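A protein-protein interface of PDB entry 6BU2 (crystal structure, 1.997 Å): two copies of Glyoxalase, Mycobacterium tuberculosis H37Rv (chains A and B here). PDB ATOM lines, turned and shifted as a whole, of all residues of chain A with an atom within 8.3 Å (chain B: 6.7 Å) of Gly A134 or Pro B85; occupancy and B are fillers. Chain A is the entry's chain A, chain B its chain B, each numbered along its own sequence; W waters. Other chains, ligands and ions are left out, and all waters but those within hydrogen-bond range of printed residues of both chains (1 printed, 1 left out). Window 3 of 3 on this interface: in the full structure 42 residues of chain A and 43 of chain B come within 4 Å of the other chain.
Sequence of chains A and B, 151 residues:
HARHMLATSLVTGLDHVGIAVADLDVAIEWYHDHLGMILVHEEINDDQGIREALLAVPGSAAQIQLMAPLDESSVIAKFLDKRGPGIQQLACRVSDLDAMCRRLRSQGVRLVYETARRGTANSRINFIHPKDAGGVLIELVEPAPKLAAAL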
ATOM      1  N   ARG A  83      12.362   7.475  28.423  1.00  0.00           N
ATOM      2  CA  ARG A  83      13.007   6.453  27.606  1.00  0.00           C
ATOM      3  C   ARG A  83      13.714   5.371  28.419  1.00  0.00           C
ATOM      4  O   ARG A  83      14.415   4.538  27.825  1.00  0.00           O
ATOM      5  CB  ARG A  83      14.004   7.103  26.635  1.00  0.00           C
ATOM      6  CG  ARG A  83      14.974   8.099  27.278  1.00  0.00           C
ATOM      7  CD  ARG A  83      16.034   8.566  26.276  1.00  0.00           C
ATOM      8  NE  ARG A  83      17.018   7.524  25.980  1.00  0.00           N
ATOM      9  CZ  ARG A  83      17.842   7.535  24.932  1.00  0.00           C
ATOM     10  NH1 ARG A  83      17.801   8.531  24.054  1.00  0.00           N
ATOM     11  NH2 ARG A  83      18.701   6.539  24.755  1.00  0.00           N
ATOM     12  N   ILE A 128      26.939  22.874  27.970  1.00  0.00           N
ATOM     13  CA  ILE A 128      26.439  23.490  26.754  1.00  0.00           C
ATOM     14  C   ILE A 128      24.938  23.298  26.714  1.00  0.00           C
ATOM     15  O   ILE A 128      24.417  22.229  27.051  1.00  0.00           O
ATOM     16  CB  ILE A 128      27.141  22.913  25.515  1.00  0.00           C
ATOM     17  CG1 ILE A 128      28.605  23.384  25.525  1.00  0.00           C
ATOM     18  CG2 ILE A 128      26.429  23.379  24.227  1.00  0.00           C
ATOM     19  CD1 ILE A 128      29.492  22.768  24.456  1.00  0.00           C
ATOM     20  N   HIS A 129      24.221  24.352  26.371  1.00  0.00           N
ATOM     21  CA  HIS A 129      22.777  24.206  26.295  1.00  0.00           C
ATOM     22  C   HIS A 129      22.423  23.082  25.323  1.00  0.00           C
ATOM     23  O   HIS A 129      22.812  23.143  24.147  1.00  0.00           O
ATOM     24  CB  HIS A 129      22.112  25.514  25.867  1.00  0.00           C
ATOM     25  CG  HIS A 129      20.660  25.563  26.202  1.00  0.00           C
ATOM     26  ND1 HIS A 129      19.767  24.614  25.747  1.00  0.00           N
ATOM     27  CD2 HIS A 129      19.952  26.407  26.988  1.00  0.00           C
ATOM     28  CE1 HIS A 129      18.563  24.891  26.219  1.00  0.00           C
ATOM     29  NE2 HIS A 129      18.650  25.970  26.978  1.00  0.00           N
ATOM     30  N   PRO A 130      21.700  22.051  25.764  1.00  0.00           N
ATOM     31  CA  PRO A 130      21.504  20.874  24.902  1.00  0.00           C
ATOM     32  C   PRO A 130      20.825  21.179  23.579  1.00  0.00           C
ATOM     33  O   PRO A 130      21.075  20.479  22.589  1.00  0.00           O
ATOM     34  CB  PRO A 130      20.649  19.942  25.775  1.00  0.00           C
ATOM     35  CG  PRO A 130      20.009  20.857  26.808  1.00  0.00           C
ATOM     36  CD  PRO A 130      21.038  21.906  27.074  1.00  0.00           C
ATOM     37  N   LYS A 131      19.977  22.197  23.514  1.00  0.00           N
ATOM     38  CA  LYS A 131      19.328  22.456  22.239  1.00  0.00           C
ATOM     39  C   LYS A 131      20.250  23.163  21.253  1.00  0.00           C
ATOM     40  O   LYS A 131      19.973  23.153  20.047  1.00  0.00           O
ATOM     41  CB  LYS A 131      18.029  23.231  22.463  1.00  0.00           C
ATOM     42  CG  LYS A 131      16.847  22.291  22.728  1.00  0.00           C
ATOM     43  CD  LYS A 131      16.890  21.091  21.757  1.00  0.00           C
ATOM     44  CE  LYS A 131      15.853  20.016  22.081  1.00  0.00           C
ATOM     45  NZ  LYS A 131      16.179  18.690  21.460  1.00  0.00           N
ATOM     46  N   ASP A 132      21.354  23.740  21.732  1.00  0.00           N
ATOM     47  CA  ASP A 132      22.385  24.246  20.829  1.00  0.00           C
ATOM     48  C   ASP A 132      23.207  23.119  20.226  1.00  0.00           C
ATOM     49  O   ASP A 132      23.800  23.280  19.153  1.00  0.00           O
ATOM     50  CB  ASP A 132      23.307  25.203  21.574  1.00  0.00           C
ATOM     51  CG  ASP A 132      22.669  26.546  21.810  1.00  0.00           C
ATOM     52  OD1 ASP A 132      21.465  26.581  22.144  1.00  0.00           O
ATOM     53  OD2 ASP A 132      23.371  27.560  21.644  1.00  0.00           O
ATOM     54  N   ALA A 133      23.281  21.990  20.921  1.00  0.00           N
ATOM     55  CA  ALA A 133      24.044  20.828  20.493  1.00  0.00           C
ATOM     56  C   ALA A 133      23.143  19.728  19.955  1.00  0.00           C
ATOM     57  O   ALA A 133      23.511  18.551  20.007  1.00  0.00           O
ATOM     58  CB  ALA A 133      24.889  20.302  21.654  1.00  0.00           C
ATOM     59  N   GLY A 134      21.953  20.090  19.468  1.00  0.00           N
ATOM     60  CA  GLY A 134      21.019  19.130  18.917  1.00  0.00           C
ATOM     61  C   GLY A 134      20.595  18.032  19.875  1.00  0.00           C
ATOM     62  O   GLY A 134      20.690  16.848  19.544  1.00  0.00           O
ATOM     63  N   GLY A 135      20.139  18.411  21.069  1.00  0.00           N
ATOM     64  CA  GLY A 135      19.651  17.464  22.052  1.00  0.00           C
ATOM     65  C   GLY A 135      20.710  16.710  22.828  1.00  0.00           C
ATOM     66  O   GLY A 135      20.370  16.036  23.806  1.00  0.00           O
ATOM     67  N   VAL A 136      21.976  16.801  22.438  1.00  0.00           N
ATOM     68  CA  VAL A 136      23.049  16.132  23.163  1.00  0.00           C
ATOM     69  C   VAL A 136      23.482  17.002  24.340  1.00  0.00           C
ATOM     70  O   VAL A 136      23.735  18.202  24.183  1.00  0.00           O
ATOM     71  CB  VAL A 136      24.227  15.843  22.223  1.00  0.00           C
ATOM     72  CG1 VAL A 136      25.395  15.245  23.003  1.00  0.00           C
ATOM     73  CG2 VAL A 136      23.774  14.908  21.086  1.00  0.00           C
ATOM     74  N   LEU A 137      23.583  16.394  25.522  1.00  0.00           N
ATOM     75  CA  LEU A 137      24.008  17.094  26.733  1.00  0.00           C
ATOM     76  C   LEU A 137      25.511  16.940  26.913  1.00  0.00           C
ATOM     77  O   LEU A 137      25.998  15.847  27.218  1.00  0.00           O
ATOM     78  CB  LEU A 137      23.270  16.547  27.950  1.00  0.00           C
ATOM     79  CG  LEU A 137      23.522  17.308  29.245  1.00  0.00           C
ATOM     80  CD1 LEU A 137      23.202  18.774  29.046  1.00  0.00           C
ATOM     81  CD2 LEU A 137      22.688  16.722  30.403  1.00  0.00           C
ATOM     82  N   ILE A 138      26.239  18.042  26.766  1.00  0.00           N
ATOM     83  CA  ILE A 138      27.685  18.067  26.895  1.00  0.00           C
ATOM     84  C   ILE A 138      28.040  18.859  28.148  1.00  0.00           C
ATOM     85  O   ILE A 138      27.750  20.059  28.252  1.00  0.00           O
ATOM     86  CB  ILE A 138      28.358  18.674  25.654  1.00  0.00           C
ATOM     87  CG1 ILE A 138      27.975  17.849  24.410  1.00  0.00           C
ATOM     88  CG2 ILE A 138      29.868  18.661  25.856  1.00  0.00           C
ATOM     89  CD1 ILE A 138      28.222  18.594  23.079  1.00  0.00           C
ATOM     90  N   ILE B  19      27.495   9.017  18.935  1.00  0.00           N
ATOM     91  CA  ILE B  19      26.447  10.031  18.974  1.00  0.00           C
ATOM     92  C   ILE B  19      25.725  10.031  17.632  1.00  0.00           C
ATOM     93  O   ILE B  19      26.352  10.231  16.584  1.00  0.00           O
ATOM     94  CB  ILE B  19      27.011  11.427  19.297  1.00  0.00           C
ATOM     95  CG1 ILE B  19      27.710  11.422  20.662  1.00  0.00           C
ATOM     96  CG2 ILE B  19      25.887  12.456  19.258  1.00  0.00           C
ATOM     97  CD1 ILE B  19      28.487  12.717  20.998  1.00  0.00           C
ATOM     98  N   ALA B  20      24.412   9.793  17.674  1.00  0.00           N
ATOM     99  CA  ALA B  20      23.543   9.915  16.508  1.00  0.00           C
ATOM    100  C   ALA B  20      23.276  11.383  16.227  1.00  0.00           C
ATOM    101  O   ALA B  20      22.811  12.110  17.117  1.00  0.00           O
ATOM    102  CB  ALA B  20      22.222   9.184  16.747  1.00  0.00           C
ATOM    103  N   VAL B  21      23.580  11.831  15.008  1.00  0.00           N
ATOM    104  CA  VAL B  21      23.313  13.213  14.618  1.00  0.00           C
ATOM    105  C   VAL B  21      22.462  13.225  13.358  1.00  0.00           C
ATOM    106  O   VAL B  21      22.364  12.238  12.632  1.00  0.00           O
ATOM    107  CB  VAL B  21      24.603  14.032  14.407  1.00  0.00           C
ATOM    108  CG1 VAL B  21      25.381  14.156  15.732  1.00  0.00           C
ATOM    109  CG2 VAL B  21      25.473  13.423  13.292  1.00  0.00           C
ATOM    110  N   ALA B  22      21.842  14.373  13.100  1.00  0.00           N
ATOM    111  CA  ALA B  22      20.966  14.486  11.939  1.00  0.00           C
ATOM    112  C   ALA B  22      21.753  14.787  10.663  1.00  0.00           C
ATOM    113  O   ALA B  22      21.424  14.264   9.593  1.00  0.00           O
ATOM    114  CB  ALA B  22      19.909  15.563  12.190  1.00  0.00           C
ATOM    115  N   TRP B  30      30.800  21.570  13.951  1.00  0.00           N
ATOM    116  CA  TRP B  30      30.382  22.076  15.257  1.00  0.00           C
ATOM    117  C   TRP B  30      31.288  21.549  16.365  1.00  0.00           C
ATOM    118  O   TRP B  30      31.806  22.325  17.179  1.00  0.00           O
ATOM    119  CB  TRP B  30      28.923  21.699  15.518  1.00  0.00           C
ATOM    120  CG  TRP B  30      28.306  22.409  16.683  1.00  0.00           C
ATOM    121  CD1 TRP B  30      27.552  23.573  16.648  1.00  0.00           C
ATOM    122  CD2 TRP B  30      28.383  22.024  18.056  1.00  0.00           C
ATOM    123  NE1 TRP B  30      27.166  23.916  17.925  1.00  0.00           N
ATOM    124  CE2 TRP B  30      27.664  22.983  18.805  1.00  0.00           C
ATOM    125  CE3 TRP B  30      28.998  20.959  18.731  1.00  0.00           C
ATOM    126  CZ2 TRP B  30      27.536  22.902  20.196  1.00  0.00           C
ATOM    127  CZ3 TRP B  30      28.877  20.888  20.114  1.00  0.00           C
ATOM    128  CH2 TRP B  30      28.153  21.853  20.828  1.00  0.00           C
ATOM    129  N   PHE B  79      16.680   5.385  16.120  1.00  0.00           N
ATOM    130  CA  PHE B  79      17.024   6.230  17.259  1.00  0.00           C
ATOM    131  C   PHE B  79      16.633   7.687  17.010  1.00  0.00           C
ATOM    132  O   PHE B  79      16.094   8.355  17.901  1.00  0.00           O
ATOM    133  CB  PHE B  79      18.523   6.087  17.545  1.00  0.00           C
ATOM    134  CG  PHE B  79      19.009   6.872  18.736  1.00  0.00           C
ATOM    135  CD1 PHE B  79      19.326   8.220  18.618  1.00  0.00           C
ATOM    136  CD2 PHE B  79      19.181   6.252  19.966  1.00  0.00           C
ATOM    137  CE1 PHE B  79      19.783   8.940  19.718  1.00  0.00           C
ATOM    138  CE2 PHE B  79      19.647   6.962  21.071  1.00  0.00           C
ATOM    139  CZ  PHE B  79      19.949   8.297  20.951  1.00  0.00           C
ATOM    140  N   LEU B  80      16.859   8.186  15.788  1.00  0.00           N
ATOM    141  CA  LEU B  80      16.590   9.591  15.492  1.00  0.00           C
ATOM    142  C   LEU B  80      15.093   9.877  15.379  1.00  0.00           C
ATOM    143  O   LEU B  80      14.638  10.974  15.731  1.00  0.00           O
ATOM    144  CB  LEU B  80      17.298  10.005  14.199  1.00  0.00           C
ATOM    145  CG  LEU B  80      18.816  10.124  14.277  1.00  0.00           C
ATOM    146  CD1 LEU B  80      19.351  10.453  12.905  1.00  0.00           C
ATOM    147  CD2 LEU B  80      19.194  11.212  15.267  1.00  0.00           C
ATOM    148  N   ARG B  83      13.828   9.817  19.361  1.00  0.00           N
ATOM    149  CA  ARG B  83      14.340  10.765  20.345  1.00  0.00           C
ATOM    150  C   ARG B  83      15.150  11.907  19.741  1.00  0.00           C
ATOM    151  O   ARG B  83      15.650  12.755  20.492  1.00  0.00           O
ATOM    152  CB  ARG B  83      15.186  10.034  21.396  1.00  0.00           C
ATOM    153  N   GLY B  84      15.290  11.967  18.417  1.00  0.00           N
ATOM    154  CA  GLY B  84      16.174  12.932  17.801  1.00  0.00           C
ATOM    155  C   GLY B  84      17.624  12.567  18.061  1.00  0.00           C
ATOM    156  O   GLY B  84      17.936  11.450  18.491  1.00  0.00           O
ATOM    157  N   PRO B  85      18.541  13.499  17.809  1.00  0.00           N
ATOM    158  CA  PRO B  85      19.957  13.217  18.075  1.00  0.00           C
ATOM    159  C   PRO B  85      20.197  12.918  19.549  1.00  0.00           C
ATOM    160  O   PRO B  85      19.488  13.398  20.432  1.00  0.00           O
ATOM    161  CB  PRO B  85      20.671  14.504  17.638  1.00  0.00           C
ATOM    162  CG  PRO B  85      19.705  15.193  16.717  1.00  0.00           C
ATOM    163  CD  PRO B  85      18.337  14.836  17.218  1.00  0.00           C
ATOM    164  N   GLY B  86      21.209  12.109  19.814  1.00  0.00           N
ATOM    165  CA  GLY B  86      21.554  11.832  21.192  1.00  0.00           C
ATOM    166  C   GLY B  86      22.704  10.857  21.260  1.00  0.00           C
ATOM    167  O   GLY B  86      23.171  10.342  20.236  1.00  0.00           O
ATOM    168  N   ILE B  87      23.134  10.581  22.491  1.00  0.00           N
ATOM    169  CA  ILE B  87      24.228   9.637  22.697  1.00  0.00           C
ATOM    170  C   ILE B  87      23.663   8.223  22.623  1.00  0.00           C
ATOM    171  O   ILE B  87      22.773   7.861  23.399  1.00  0.00           O
ATOM    172  CB  ILE B  87      24.930   9.875  24.040  1.00  0.00           C
ATOM    173  CG1 ILE B  87      25.249  11.360  24.233  1.00  0.00           C
ATOM    174  CG2 ILE B  87      26.167   8.979  24.092  1.00  0.00           C
ATOM    175  CD1 ILE B  87      25.789  11.730  25.643  1.00  0.00           C
HETATM  176  O   HOH W   1      21.527   5.648  25.401  1.00  0.00           O
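The backbone NH of Ile A128 lies within hydrogen-bond range of the backbone carbonyl oxygen of Ile A138 (2.9 Å).
The backbone NH (N) of Ala B20 lies within hydrogen-bond range of the backbone carbonyl oxygen (O) of Gly B86 (2.9 Å).
Of the 12 printed residues of chain A, 7 touch a printed residue of chain B.
Hydrophobic or aromatic side chains of chain A within 4 Å of the printed part of chain B: Ile A128, Ala A133, Val A136 and Ile A138.
Printed residues of chain B that touch a printed residue of chain A: Ile B19, Trp B30, Phe B79, Pro B85 and Gly B86.
Hydrophobic or aromatic side chains of chain B within 4 Å of the printed part of chain A: Ile B19, Trp B30, Phe B79 and Pro B85.
Along chain B the printed residues that touch a printed residue of chain A span positions 19 to 86.
Among the printed residues, no Asp or Glu carboxylate lies within 4 Å of a Lys or Arg side-chain nitrogen of the other chain.
1 position is printed for both chains.
Of the 8 pairs that touch across the chains among the printed residues, none has its exchanged pair printed and touching as well.
NH1 of Arg A83 touches CZ of Phe B79, at 3.8 Å.
CH2 of Trp B30 touches CD1 of Ile A128 (3.97 Å).
NE1 of Trp B30 touches O of Asp A132, 3.6 Å away.
CH2 of Trp B30 touches CB of Ala A133, at 3.7 Å.
Gly A134 touches Pro B85 (O to CB, 3.0 Å).
CG2 of Val A136 touches CG2 of Ile B19, 3.7 Å away.
CG2 of Val A136 touches CA of Gly B86, 3.8 Å away.
CD1 of Ile A138 touches CZ3 of Trp B30 (3.8 Å).
Pro B85 touches just one residue of chain A: Gly A134 (3.0 Å).
No residue of chain A comes within 4 Å of Gly B84.
Of the printed residues of chain A, Gly B86 touches Val A136.
Printed residues of chain A within 4 Å of Trp B30: Ile A128 (3.97 Å), Asp A132 (3.6 Å), Ala A133 (3.7 Å) and Ile A138 (3.8 Å).
Of the printed residues of chain B, Arg A83 touches Phe B79.
Of the printed residues of chain A, Ile B19 touches Val A136 (3.7 Å).
Of the printed residues of chain B, Ala A133 touches Trp B30 (3.7 Å).
Printed residues of chain B within 4 Å of Ile A128: Trp B30 (3.97 Å).
Pro A130 touches none of the printed residues of chain B.
The nearest residue of chain B that does not touch Gly A134 is Gly B86 (4.8 Å).
The nearest residue of chain A that does not touch Pro B85 is Gly A135 (4.3 Å).
The nearest printed residue of chain A that does not touch Trp B30 is His A129 (6.2 Å).
Water W1 bridges the guanidinium group of Arg A83 (3.0 Å) and the backbone carbonyl oxygen of Ile B87 (3.2 Å).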
